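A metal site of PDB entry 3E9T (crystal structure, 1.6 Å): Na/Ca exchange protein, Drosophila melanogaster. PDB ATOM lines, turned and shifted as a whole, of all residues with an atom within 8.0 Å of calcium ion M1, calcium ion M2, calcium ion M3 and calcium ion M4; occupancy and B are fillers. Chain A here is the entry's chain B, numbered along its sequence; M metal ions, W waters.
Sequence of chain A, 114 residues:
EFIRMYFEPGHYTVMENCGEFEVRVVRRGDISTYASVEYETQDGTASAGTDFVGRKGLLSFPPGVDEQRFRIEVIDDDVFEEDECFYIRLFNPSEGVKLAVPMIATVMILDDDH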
ATOM      1  N   MET A  15      27.757  -3.663  31.539  1.00  0.00           N
ATOM      2  CA  MET A  15      26.627  -4.141  30.788  1.00  0.00           C
ATOM      3  C   MET A  15      25.823  -2.955  30.261  1.00  0.00           C
ATOM      4  O   MET A  15      25.710  -1.927  30.949  1.00  0.00           O
ATOM      5  CB  MET A  15      25.728  -4.997  31.693  1.00  0.00           C
ATOM      6  CG  MET A  15      26.384  -6.238  32.276  1.00  0.00           C
ATOM      7  SD  MET A  15      27.304  -7.220  31.084  1.00  0.00           S
ATOM      8  CE  MET A  15      26.018  -7.934  30.080  1.00  0.00           C
ATOM      9  N   GLU A  16      25.235  -3.111  29.087  1.00  0.00           N
ATOM     10  CA  GLU A  16      24.426  -2.045  28.489  1.00  0.00           C
ATOM     11  C   GLU A  16      23.278  -1.597  29.389  1.00  0.00           C
ATOM     12  O   GLU A  16      22.877  -0.444  29.332  1.00  0.00           O
ATOM     13  CB  GLU A  16      23.881  -2.474  27.136  1.00  0.00           C
ATOM     14  CG  GLU A  16      23.217  -1.309  26.433  1.00  0.00           C
ATOM     15  CD  GLU A  16      22.589  -1.701  25.120  1.00  0.00           C
ATOM     16  OE1 GLU A  16      22.883  -1.029  24.108  1.00  0.00           O
ATOM     17  OE2 GLU A  16      21.806  -2.662  25.101  1.00  0.00           O
ATOM     18  N   ASN A  17      22.754  -2.507  30.215  1.00  0.00           N
ATOM     19  CA  ASN A  17      21.647  -2.182  31.116  1.00  0.00           C
ATOM     20  C   ASN A  17      22.061  -1.795  32.545  1.00  0.00           C
ATOM     21  O   ASN A  17      21.243  -1.860  33.466  1.00  0.00           O
ATOM     22  CB  ASN A  17      20.628  -3.326  31.142  1.00  0.00           C
ATOM     23  CG  ASN A  17      21.215  -4.630  31.661  1.00  0.00           C
ATOM     24  OD1 ASN A  17      22.444  -4.781  31.757  1.00  0.00           O
ATOM     25  ND2 ASN A  17      20.352  -5.565  32.010  1.00  0.00           N
ATOM     26  N   CYS A  18      23.321  -1.368  32.727  1.00  0.00           N
ATOM     27  CA  CYS A  18      23.840  -1.017  34.053  1.00  0.00           C
ATOM     28  C   CYS A  18      23.272   0.308  34.594  1.00  0.00           C
ATOM     29  O   CYS A  18      23.343   0.570  35.802  1.00  0.00           O
ATOM     30  CB  CYS A  18      25.373  -0.946  34.038  1.00  0.00           C
ATOM     31  SG  CYS A  18      26.073   0.476  33.206  1.00  0.00           S
ATOM     32  N   THR A  45      34.181   2.679  19.155  1.00  0.00           N
ATOM     33  CA  THR A  45      33.105   2.017  18.405  1.00  0.00           C
ATOM     34  C   THR A  45      31.745   2.264  19.059  1.00  0.00           C
ATOM     35  O   THR A  45      30.708   2.157  18.396  1.00  0.00           O
ATOM     36  CB  THR A  45      33.365   0.506  18.219  1.00  0.00           C
ATOM     37  OG1 THR A  45      33.763  -0.074  19.465  1.00  0.00           O
ATOM     38  CG2 THR A  45      34.468   0.298  17.191  1.00  0.00           C
ATOM     39  N   ALA A  46      31.750   2.592  20.354  1.00  0.00           N
ATOM     40  CA  ALA A  46      30.551   3.083  21.042  1.00  0.00           C
ATOM     41  C   ALA A  46      30.506   4.618  20.963  1.00  0.00           C
ATOM     42  O   ALA A  46      31.552   5.282  21.029  1.00  0.00           O
ATOM     43  CB  ALA A  46      30.549   2.624  22.485  1.00  0.00           C
ATOM     44  N   SER A  47      29.307   5.174  20.833  1.00  0.00           N
ATOM     45  CA  SER A  47      29.159   6.598  20.511  1.00  0.00           C
ATOM     46  C   SER A  47      28.288   7.358  21.493  1.00  0.00           C
ATOM     47  O   SER A  47      27.239   6.852  21.899  1.00  0.00           O
ATOM     48  CB  SER A  47      28.562   6.742  19.116  1.00  0.00           C
ATOM     49  OG  SER A  47      29.373   6.084  18.165  1.00  0.00           O
ATOM     50  N   THR A  50      24.216   7.502  21.560  1.00  0.00           N
ATOM     51  CA  THR A  50      23.600   6.233  21.187  1.00  0.00           C
ATOM     52  C   THR A  50      23.908   5.132  22.220  1.00  0.00           C
ATOM     53  O   THR A  50      23.024   4.376  22.600  1.00  0.00           O
ATOM     54  CB  THR A  50      23.956   5.771  19.736  1.00  0.00           C
ATOM     55  OG1 THR A  50      25.321   5.406  19.662  1.00  0.00           O
ATOM     56  CG2 THR A  50      23.728   6.872  18.720  1.00  0.00           C
ATOM     57  N   ASP A  51      25.153   5.081  22.695  1.00  0.00           N
ATOM     58  CA  ASP A  51      25.610   4.029  23.616  1.00  0.00           C
ATOM     59  C   ASP A  51      25.873   4.498  25.034  1.00  0.00           C
ATOM     60  O   ASP A  51      25.803   3.716  25.989  1.00  0.00           O
ATOM     61  CB  ASP A  51      26.877   3.365  23.070  1.00  0.00           C
ATOM     62  CG  ASP A  51      26.656   2.763  21.716  1.00  0.00           C
ATOM     63  OD1 ASP A  51      27.252   3.261  20.745  1.00  0.00           O
ATOM     64  OD2 ASP A  51      25.838   1.822  21.639  1.00  0.00           O
ATOM     65  N   PHE A  52      26.199   5.777  25.178  1.00  0.00           N
ATOM     66  CA  PHE A  52      26.438   6.340  26.502  1.00  0.00           C
ATOM     67  C   PHE A  52      26.138   7.817  26.404  1.00  0.00           C
ATOM     68  O   PHE A  52      26.072   8.349  25.316  1.00  0.00           O
ATOM     69  CB  PHE A  52      27.883   6.120  26.965  1.00  0.00           C
ATOM     70  CG  PHE A  52      28.942   6.777  26.063  1.00  0.00           C
ATOM     71  CD1 PHE A  52      29.453   6.100  24.944  1.00  0.00           C
ATOM     72  CD2 PHE A  52      29.419   8.045  26.340  1.00  0.00           C
ATOM     73  CE1 PHE A  52      30.411   6.694  24.100  1.00  0.00           C
ATOM     74  CE2 PHE A  52      30.388   8.643  25.505  1.00  0.00           C
ATOM     75  CZ  PHE A  52      30.890   7.947  24.404  1.00  0.00           C
ATOM     76  N   VAL A  74      25.037   4.947  30.851  1.00  0.00           N
ATOM     77  CA  VAL A  74      25.082   4.039  29.706  1.00  0.00           C
ATOM     78  C   VAL A  74      23.649   3.922  29.152  1.00  0.00           C
ATOM     79  O   VAL A  74      22.673   3.844  29.924  1.00  0.00           O
ATOM     80  CB  VAL A  74      25.671   2.667  30.125  1.00  0.00           C
ATOM     81  CG1 VAL A  74      25.632   1.672  28.959  1.00  0.00           C
ATOM     82  CG2 VAL A  74      27.137   2.835  30.617  1.00  0.00           C
ATOM     83  N   ILE A  75      23.538   4.001  27.824  1.00  0.00           N
ATOM     84  CA  ILE A  75      22.225   3.996  27.156  1.00  0.00           C
ATOM     85  C   ILE A  75      21.799   2.573  26.802  1.00  0.00           C
ATOM     86  O   ILE A  75      22.490   1.855  26.093  1.00  0.00           O
ATOM     87  CB  ILE A  75      22.174   4.940  25.908  1.00  0.00           C
ATOM     88  CG1 ILE A  75      22.473   6.390  26.325  1.00  0.00           C
ATOM     89  CG2 ILE A  75      20.796   4.823  25.192  1.00  0.00           C
ATOM     90  CD1 ILE A  75      22.579   7.374  25.157  1.00  0.00           C
ATOM     91  N   ASP A  76      20.636   2.174  27.324  1.00  0.00           N
ATOM     92  CA  ASP A  76      20.113   0.854  27.069  1.00  0.00           C
ATOM     93  C   ASP A  76      19.178   0.912  25.872  1.00  0.00           C
ATOM     94  O   ASP A  76      18.412   1.853  25.728  1.00  0.00           O
ATOM     95  CB  ASP A  76      19.347   0.342  28.304  1.00  0.00           C
ATOM     96  CG  ASP A  76      19.099  -1.156  28.273  1.00  0.00           C
ATOM     97  OD1 ASP A  76      18.317  -1.632  29.116  1.00  0.00           O
ATOM     98  OD2 ASP A  76      19.690  -1.860  27.427  1.00  0.00           O
ATOM     99  N   ASP A  77      19.253  -0.085  25.009  1.00  0.00           N
ATOM    100  CA  ASP A  77      18.198  -0.257  24.000  1.00  0.00           C
ATOM    101  C   ASP A  77      17.779  -1.719  23.862  1.00  0.00           C
ATOM    102  O   ASP A  77      18.173  -2.569  24.670  1.00  0.00           O
ATOM    103  CB  ASP A  77      18.554   0.397  22.653  1.00  0.00           C
ATOM    104  CG  ASP A  77      19.845  -0.117  22.058  1.00  0.00           C
ATOM    105  OD1 ASP A  77      20.563   0.692  21.432  1.00  0.00           O
ATOM    106  OD2 ASP A  77      20.146  -1.317  22.201  1.00  0.00           O
ATOM    107  N   ASP A  78      16.942  -2.002  22.865  1.00  0.00           N
ATOM    108  CA  ASP A  78      16.446  -3.351  22.647  1.00  0.00           C
ATOM    109  C   ASP A  78      17.120  -3.978  21.432  1.00  0.00           C
ATOM    110  O   ASP A  78      16.746  -5.072  20.989  1.00  0.00           O
ATOM    111  CB  ASP A  78      14.916  -3.320  22.428  1.00  0.00           C
ATOM    112  CG  ASP A  78      14.137  -3.009  23.709  1.00  0.00           C
ATOM    113  OD1 ASP A  78      14.762  -2.707  24.763  1.00  0.00           O
ATOM    114  OD2 ASP A  78      12.883  -3.069  23.665  1.00  0.00           O
ATOM    115  N   VAL A  79      18.121  -3.274  20.896  1.00  0.00           N
ATOM    116  CA  VAL A  79      18.839  -3.707  19.707  1.00  0.00           C
ATOM    117  C   VAL A  79      20.098  -4.479  20.112  1.00  0.00           C
ATOM    118  O   VAL A  79      20.928  -3.990  20.880  1.00  0.00           O
ATOM    119  CB  VAL A  79      19.249  -2.488  18.831  1.00  0.00           C
ATOM    120  CG1 VAL A  79      19.926  -2.941  17.550  1.00  0.00           C
ATOM    121  CG2 VAL A  79      18.018  -1.621  18.502  1.00  0.00           C
ATOM    122  N   PHE A  80      20.229  -5.700  19.577  1.00  0.00           N
ATOM    123  CA  PHE A  80      21.452  -6.477  19.750  1.00  0.00           C
ATOM    124  C   PHE A  80      22.645  -5.740  19.138  1.00  0.00           C
ATOM    125  O   PHE A  80      22.549  -5.205  18.028  1.00  0.00           O
ATOM    126  CB  PHE A  80      21.304  -7.858  19.094  1.00  0.00           C
ATOM    127  CG  PHE A  80      22.606  -8.464  18.665  1.00  0.00           C
ATOM    128  CD1 PHE A  80      22.992  -8.437  17.328  1.00  0.00           C
ATOM    129  CD2 PHE A  80      23.473  -9.025  19.603  1.00  0.00           C
ATOM    130  CE1 PHE A  80      24.215  -8.981  16.924  1.00  0.00           C
ATOM    131  CE2 PHE A  80      24.699  -9.572  19.209  1.00  0.00           C
ATOM    132  CZ  PHE A  80      25.061  -9.548  17.867  1.00  0.00           C
ATOM    133  N   GLU A  81      23.742  -5.695  19.893  1.00  0.00           N
ATOM    134  CA  GLU A  81      25.024  -5.142  19.400  1.00  0.00           C
ATOM    135  C   GLU A  81      26.216  -6.003  19.833  1.00  0.00           C
ATOM    136  O   GLU A  81      26.156  -6.684  20.850  1.00  0.00           O
ATOM    137  CB  GLU A  81      25.261  -3.719  19.919  1.00  0.00           C
ATOM    138  CG  GLU A  81      24.175  -2.715  19.562  1.00  0.00           C
ATOM    139  CD  GLU A  81      24.086  -1.630  20.591  1.00  0.00           C
ATOM    140  OE1 GLU A  81      23.169  -1.693  21.446  1.00  0.00           O
ATOM    141  OE2 GLU A  81      24.956  -0.724  20.584  1.00  0.00           O
ATOM    142  N   GLU A  82      27.303  -5.929  19.078  1.00  0.00           N
ATOM    143  CA  GLU A  82      28.548  -6.566  19.453  1.00  0.00           C
ATOM    144  C   GLU A  82      29.217  -5.776  20.593  1.00  0.00           C
ATOM    145  O   GLU A  82      28.761  -4.670  20.915  1.00  0.00           O
ATOM    146  CB  GLU A  82      29.450  -6.648  18.225  1.00  0.00           C
ATOM    147  CG  GLU A  82      28.715  -7.290  17.034  1.00  0.00           C
ATOM    148  CD  GLU A  82      29.585  -7.519  15.814  1.00  0.00           C
ATOM    149  OE1 GLU A  82      29.075  -8.099  14.831  1.00  0.00           O
ATOM    150  OE2 GLU A  82      30.774  -7.113  15.814  1.00  0.00           O
ATOM    151  N   ASP A  83      30.264  -6.322  21.209  1.00  0.00           N
ATOM    152  CA  ASP A  83      30.984  -5.568  22.243  1.00  0.00           C
ATOM    153  C   ASP A  83      31.547  -4.294  21.608  1.00  0.00           C
ATOM    154  O   ASP A  83      32.128  -4.349  20.532  1.00  0.00           O
ATOM    155  CB  ASP A  83      32.154  -6.346  22.842  1.00  0.00           C
ATOM    156  CG  ASP A  83      31.710  -7.613  23.560  1.00  0.00           C
ATOM    157  OD1 ASP A  83      30.481  -7.841  23.685  1.00  0.00           O
ATOM    158  OD2 ASP A  83      32.594  -8.411  23.985  1.00  0.00           O
ATOM    159  N   GLU A  84      31.380  -3.160  22.283  1.00  0.00           N
ATOM    160  CA  GLU A  84      31.875  -1.877  21.752  1.00  0.00           C
ATOM    161  C   GLU A  84      32.592  -1.100  22.838  1.00  0.00           C
ATOM    162  O   GLU A  84      32.284  -1.260  24.006  1.00  0.00           O
ATOM    163  CB  GLU A  84      30.746  -1.037  21.180  1.00  0.00           C
ATOM    164  CG  GLU A  84      30.063  -1.693  19.989  1.00  0.00           C
ATOM    165  CD  GLU A  84      28.966  -0.846  19.376  1.00  0.00           C
ATOM    166  OE1 GLU A  84      28.355  -0.022  20.091  1.00  0.00           O
ATOM    167  OE2 GLU A  84      28.710  -1.033  18.167  1.00  0.00           O
ATOM    168  N   ILE A 109      31.450  -1.889  26.596  1.00  0.00           N
ATOM    169  CA  ILE A 109      30.047  -2.091  26.866  1.00  0.00           C
ATOM    170  C   ILE A 109      29.667  -3.447  26.275  1.00  0.00           C
ATOM    171  O   ILE A 109      29.886  -3.704  25.080  1.00  0.00           O
ATOM    172  CB  ILE A 109      29.141  -0.994  26.224  1.00  0.00           C
ATOM    173  CG1 ILE A 109      29.475   0.407  26.724  1.00  0.00           C
ATOM    174  CG2 ILE A 109      27.633  -1.319  26.502  1.00  0.00           C
ATOM    175  CD1 ILE A 109      28.821   1.521  25.880  1.00  0.00           C
ATOM    176  N   LEU A 110      29.108  -4.299  27.120  1.00  0.00           N
ATOM    177  CA  LEU A 110      28.601  -5.604  26.699  1.00  0.00           C
ATOM    178  C   LEU A 110      27.094  -5.533  26.562  1.00  0.00           C
ATOM    179  O   LEU A 110      26.423  -5.023  27.451  1.00  0.00           O
ATOM    180  CB  LEU A 110      28.959  -6.686  27.721  1.00  0.00           C
ATOM    181  CG  LEU A 110      30.419  -6.726  28.192  1.00  0.00           C
ATOM    182  CD1 LEU A 110      30.587  -7.851  29.188  1.00  0.00           C
ATOM    183  CD2 LEU A 110      31.391  -6.871  26.997  1.00  0.00           C
ATOM    184  N   ASP A 111      26.577  -6.023  25.445  1.00  0.00           N
ATOM    185  CA  ASP A 111      25.147  -5.961  25.146  1.00  0.00           C
ATOM    186  C   ASP A 111      24.388  -7.013  25.952  1.00  0.00           C
ATOM    187  O   ASP A 111      24.949  -8.055  26.310  1.00  0.00           O
ATOM    188  CB  ASP A 111      24.924  -6.160  23.646  1.00  0.00           C
ATOM    189  CG  ASP A 111      23.597  -5.605  23.151  1.00  0.00           C
ATOM    190  OD1 ASP A 111      23.477  -4.371  22.968  1.00  0.00           O
ATOM    191  OD2 ASP A 111      22.684  -6.403  22.898  1.00  0.00           O
ATOM    192  N   ASP A 112      23.110  -6.750  26.218  1.00  0.00           N
ATOM    193  CA  ASP A 112      22.245  -7.670  26.969  1.00  0.00           C
ATOM    194  C   ASP A 112      21.052  -8.188  26.151  1.00  0.00           C
ATOM    195  O   ASP A 112      20.257  -8.993  26.639  1.00  0.00           O
ATOM    196  CB  ASP A 112      21.740  -6.988  28.254  1.00  0.00           C
ATOM    197  CG  ASP A 112      20.884  -5.756  27.958  1.00  0.00           C
ATOM    198  OD1 ASP A 112      21.235  -4.959  27.056  1.00  0.00           O
ATOM    199  OD2 ASP A 112      19.842  -5.568  28.628  1.00  0.00           O
ATOM    200  N   ASP A 113      20.948  -7.731  24.897  1.00  0.00           N
ATOM    201  CA  ASP A 113      19.780  -7.991  24.042  1.00  0.00           C
ATOM    202  C   ASP A 113      19.897  -9.277  23.216  1.00  0.00           C
ATOM    203  O   ASP A 113      20.664  -9.355  22.244  1.00  0.00           O
ATOM    204  CB  ASP A 113      19.516  -6.781  23.129  1.00  0.00           C
ATOM    205  CG  ASP A 113      19.459  -5.475  23.909  1.00  0.00           C
ATOM    206  OD1 ASP A 113      18.715  -5.435  24.926  1.00  0.00           O
ATOM    207  OD2 ASP A 113      20.133  -4.493  23.529  1.00  0.00           O
HETATM  208 CA    CA M   1      19.556  -3.564  26.088  1.00  0.00          CA
HETATM  209 CA    CA M   2      21.526  -3.097  22.772  1.00  0.00          CA
HETATM  210 CA    CA M   3      24.758  -0.135  22.971  1.00  0.00          CA
HETATM  211 CA    CA M   4      26.173   1.033  19.296  1.00  0.00          CA
HETATM  212  O   HOH W   1      25.219   0.089  17.376  1.00  0.00           O
HETATM  213  O   HOH W   2      27.581   2.085  18.225  1.00  0.00           O
HETATM  214  O   HOH W   3      22.985   1.276  22.416  1.00  0.00           O
HETATM  215  O   HOH W   4      25.339  -2.779  23.770  1.00  0.00           O
HETATM  216  O   HOH W   5      27.397  -0.466  22.870  1.00  0.00           O
HETATM  217  O   HOH W   6      25.038   1.139  25.315  1.00  0.00           O
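The backbone carbonyl oxygen (O) of Leu 110 sits at hydrogen-bond distance from the backbone NH (N) of Glu 16, at 2.8 Å.
The side-chain carboxylate (OD2) of Asp 112 sits at hydrogen-bond distance from the side-chain amide nitrogen (ND2) of Asn 17 (3.4 Å).
O of Asp 51 is in hydrogen-bond range of N of Ile 75, 2.9 Å away.
OG1 of Thr 50 lies close to OD1 of Asp 51 (3.1 Å).
OD1 of Asp 51 sits close to N of Ser 47.
The backbone NH (N) of Ile 109 sits at hydrogen-bond distance from the backbone carbonyl oxygen (O) of Glu 84 (2.8 Å).
Five residues have an atom within 4 Å of calcium ion M1: Glu 16, Asp 76, Asp 77, Asp 112 and Asp 113.
The nearest printed residue that does not touch calcium ion M1 is Asp 78 (4.4 Å).
Along chain A the residues within 4 Å of calcium ion M2 span positions 16 to 113.
The nearest printed residue that does not touch calcium ion M2 is Phe 80 (4.3 Å).
Of the 26 residues printed, 3 come within 4 Å of calcium ion M3.
The nearest printed residue that does not touch calcium ion M3 is Ile 75 (4.3 Å).
Of the 26 residues printed, 3 come within 4 Å of calcium ion M4.
Calcium ion M1 is bound by the side-chain carboxylate (OD2) of Asp 76 (2.2 Å), the backbone carbonyl oxygen (O) of Asp 77 (2.2 Å), the side-chain carboxylate (OD1) of Asp 113 (2.4 Å), the side-chain carboxylate (OD1) of Asp 112 (2.4 Å), the side-chain carboxylate (OE2) of Glu 16 (2.6 Å) and the side-chain carboxylate (OD2) of Asp 113 (2.8 Å).
Calcium ion M1 has six donor atoms within binding distance.
The side-chain carboxylate (OD2) of Asp 113 binds calcium ion M2, 2.1 Å away.
O of Val 79 is bound to calcium ion M2, 2.2 Å away.
OD2 of Asp 77 is bound to calcium ion M2 (2.3 Å).
OD1 of Asp 111 is bound to calcium ion M2, 2.3 Å away.
OE2 of Glu 16 binds calcium ion M2 (2.4 Å).
OE1 of Glu 81 is bound to calcium ion M2, 2.5 Å away.
Calcium ion M2 is bound by OE1 of Glu 16, 2.8 Å away.
Calcium ion M3 is bound by water W3 (2.3 Å), the side-chain carboxylate (OE1) of Glu 16 (2.4 Å), the side-chain carboxylate (OE2) of Glu 81 (2.5 Å), the side-chain carboxylate (OD2) of Asp 51 (2.6 Å), water W5 (2.7 Å), water W6 (2.7 Å), the side-chain carboxylate (OE1) of Glu 81 (2.7 Å) and water W4 (2.8 Å).
Calcium ion M3 has eight donor atoms within binding distance.
Calcium ion M4 is bound by water W2, water W1, OD2 of Asp 51, OE2 of Glu 81, OE1 of Glu 84 and OD1 of Asp 51.
Calcium ion M4 has six donor atoms within binding distance.
Water W6 bridges the backbone carbonyl oxygen (O) of Ile 75 and the backbone carbonyl oxygen (O) of Asp 51.
Water W3 bridges OD1 of Asp 77 (2.7 Å) and O of Thr 50 (3.1 Å).
Water W2 bridges O of Thr 45 and OE2 of Glu 84.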
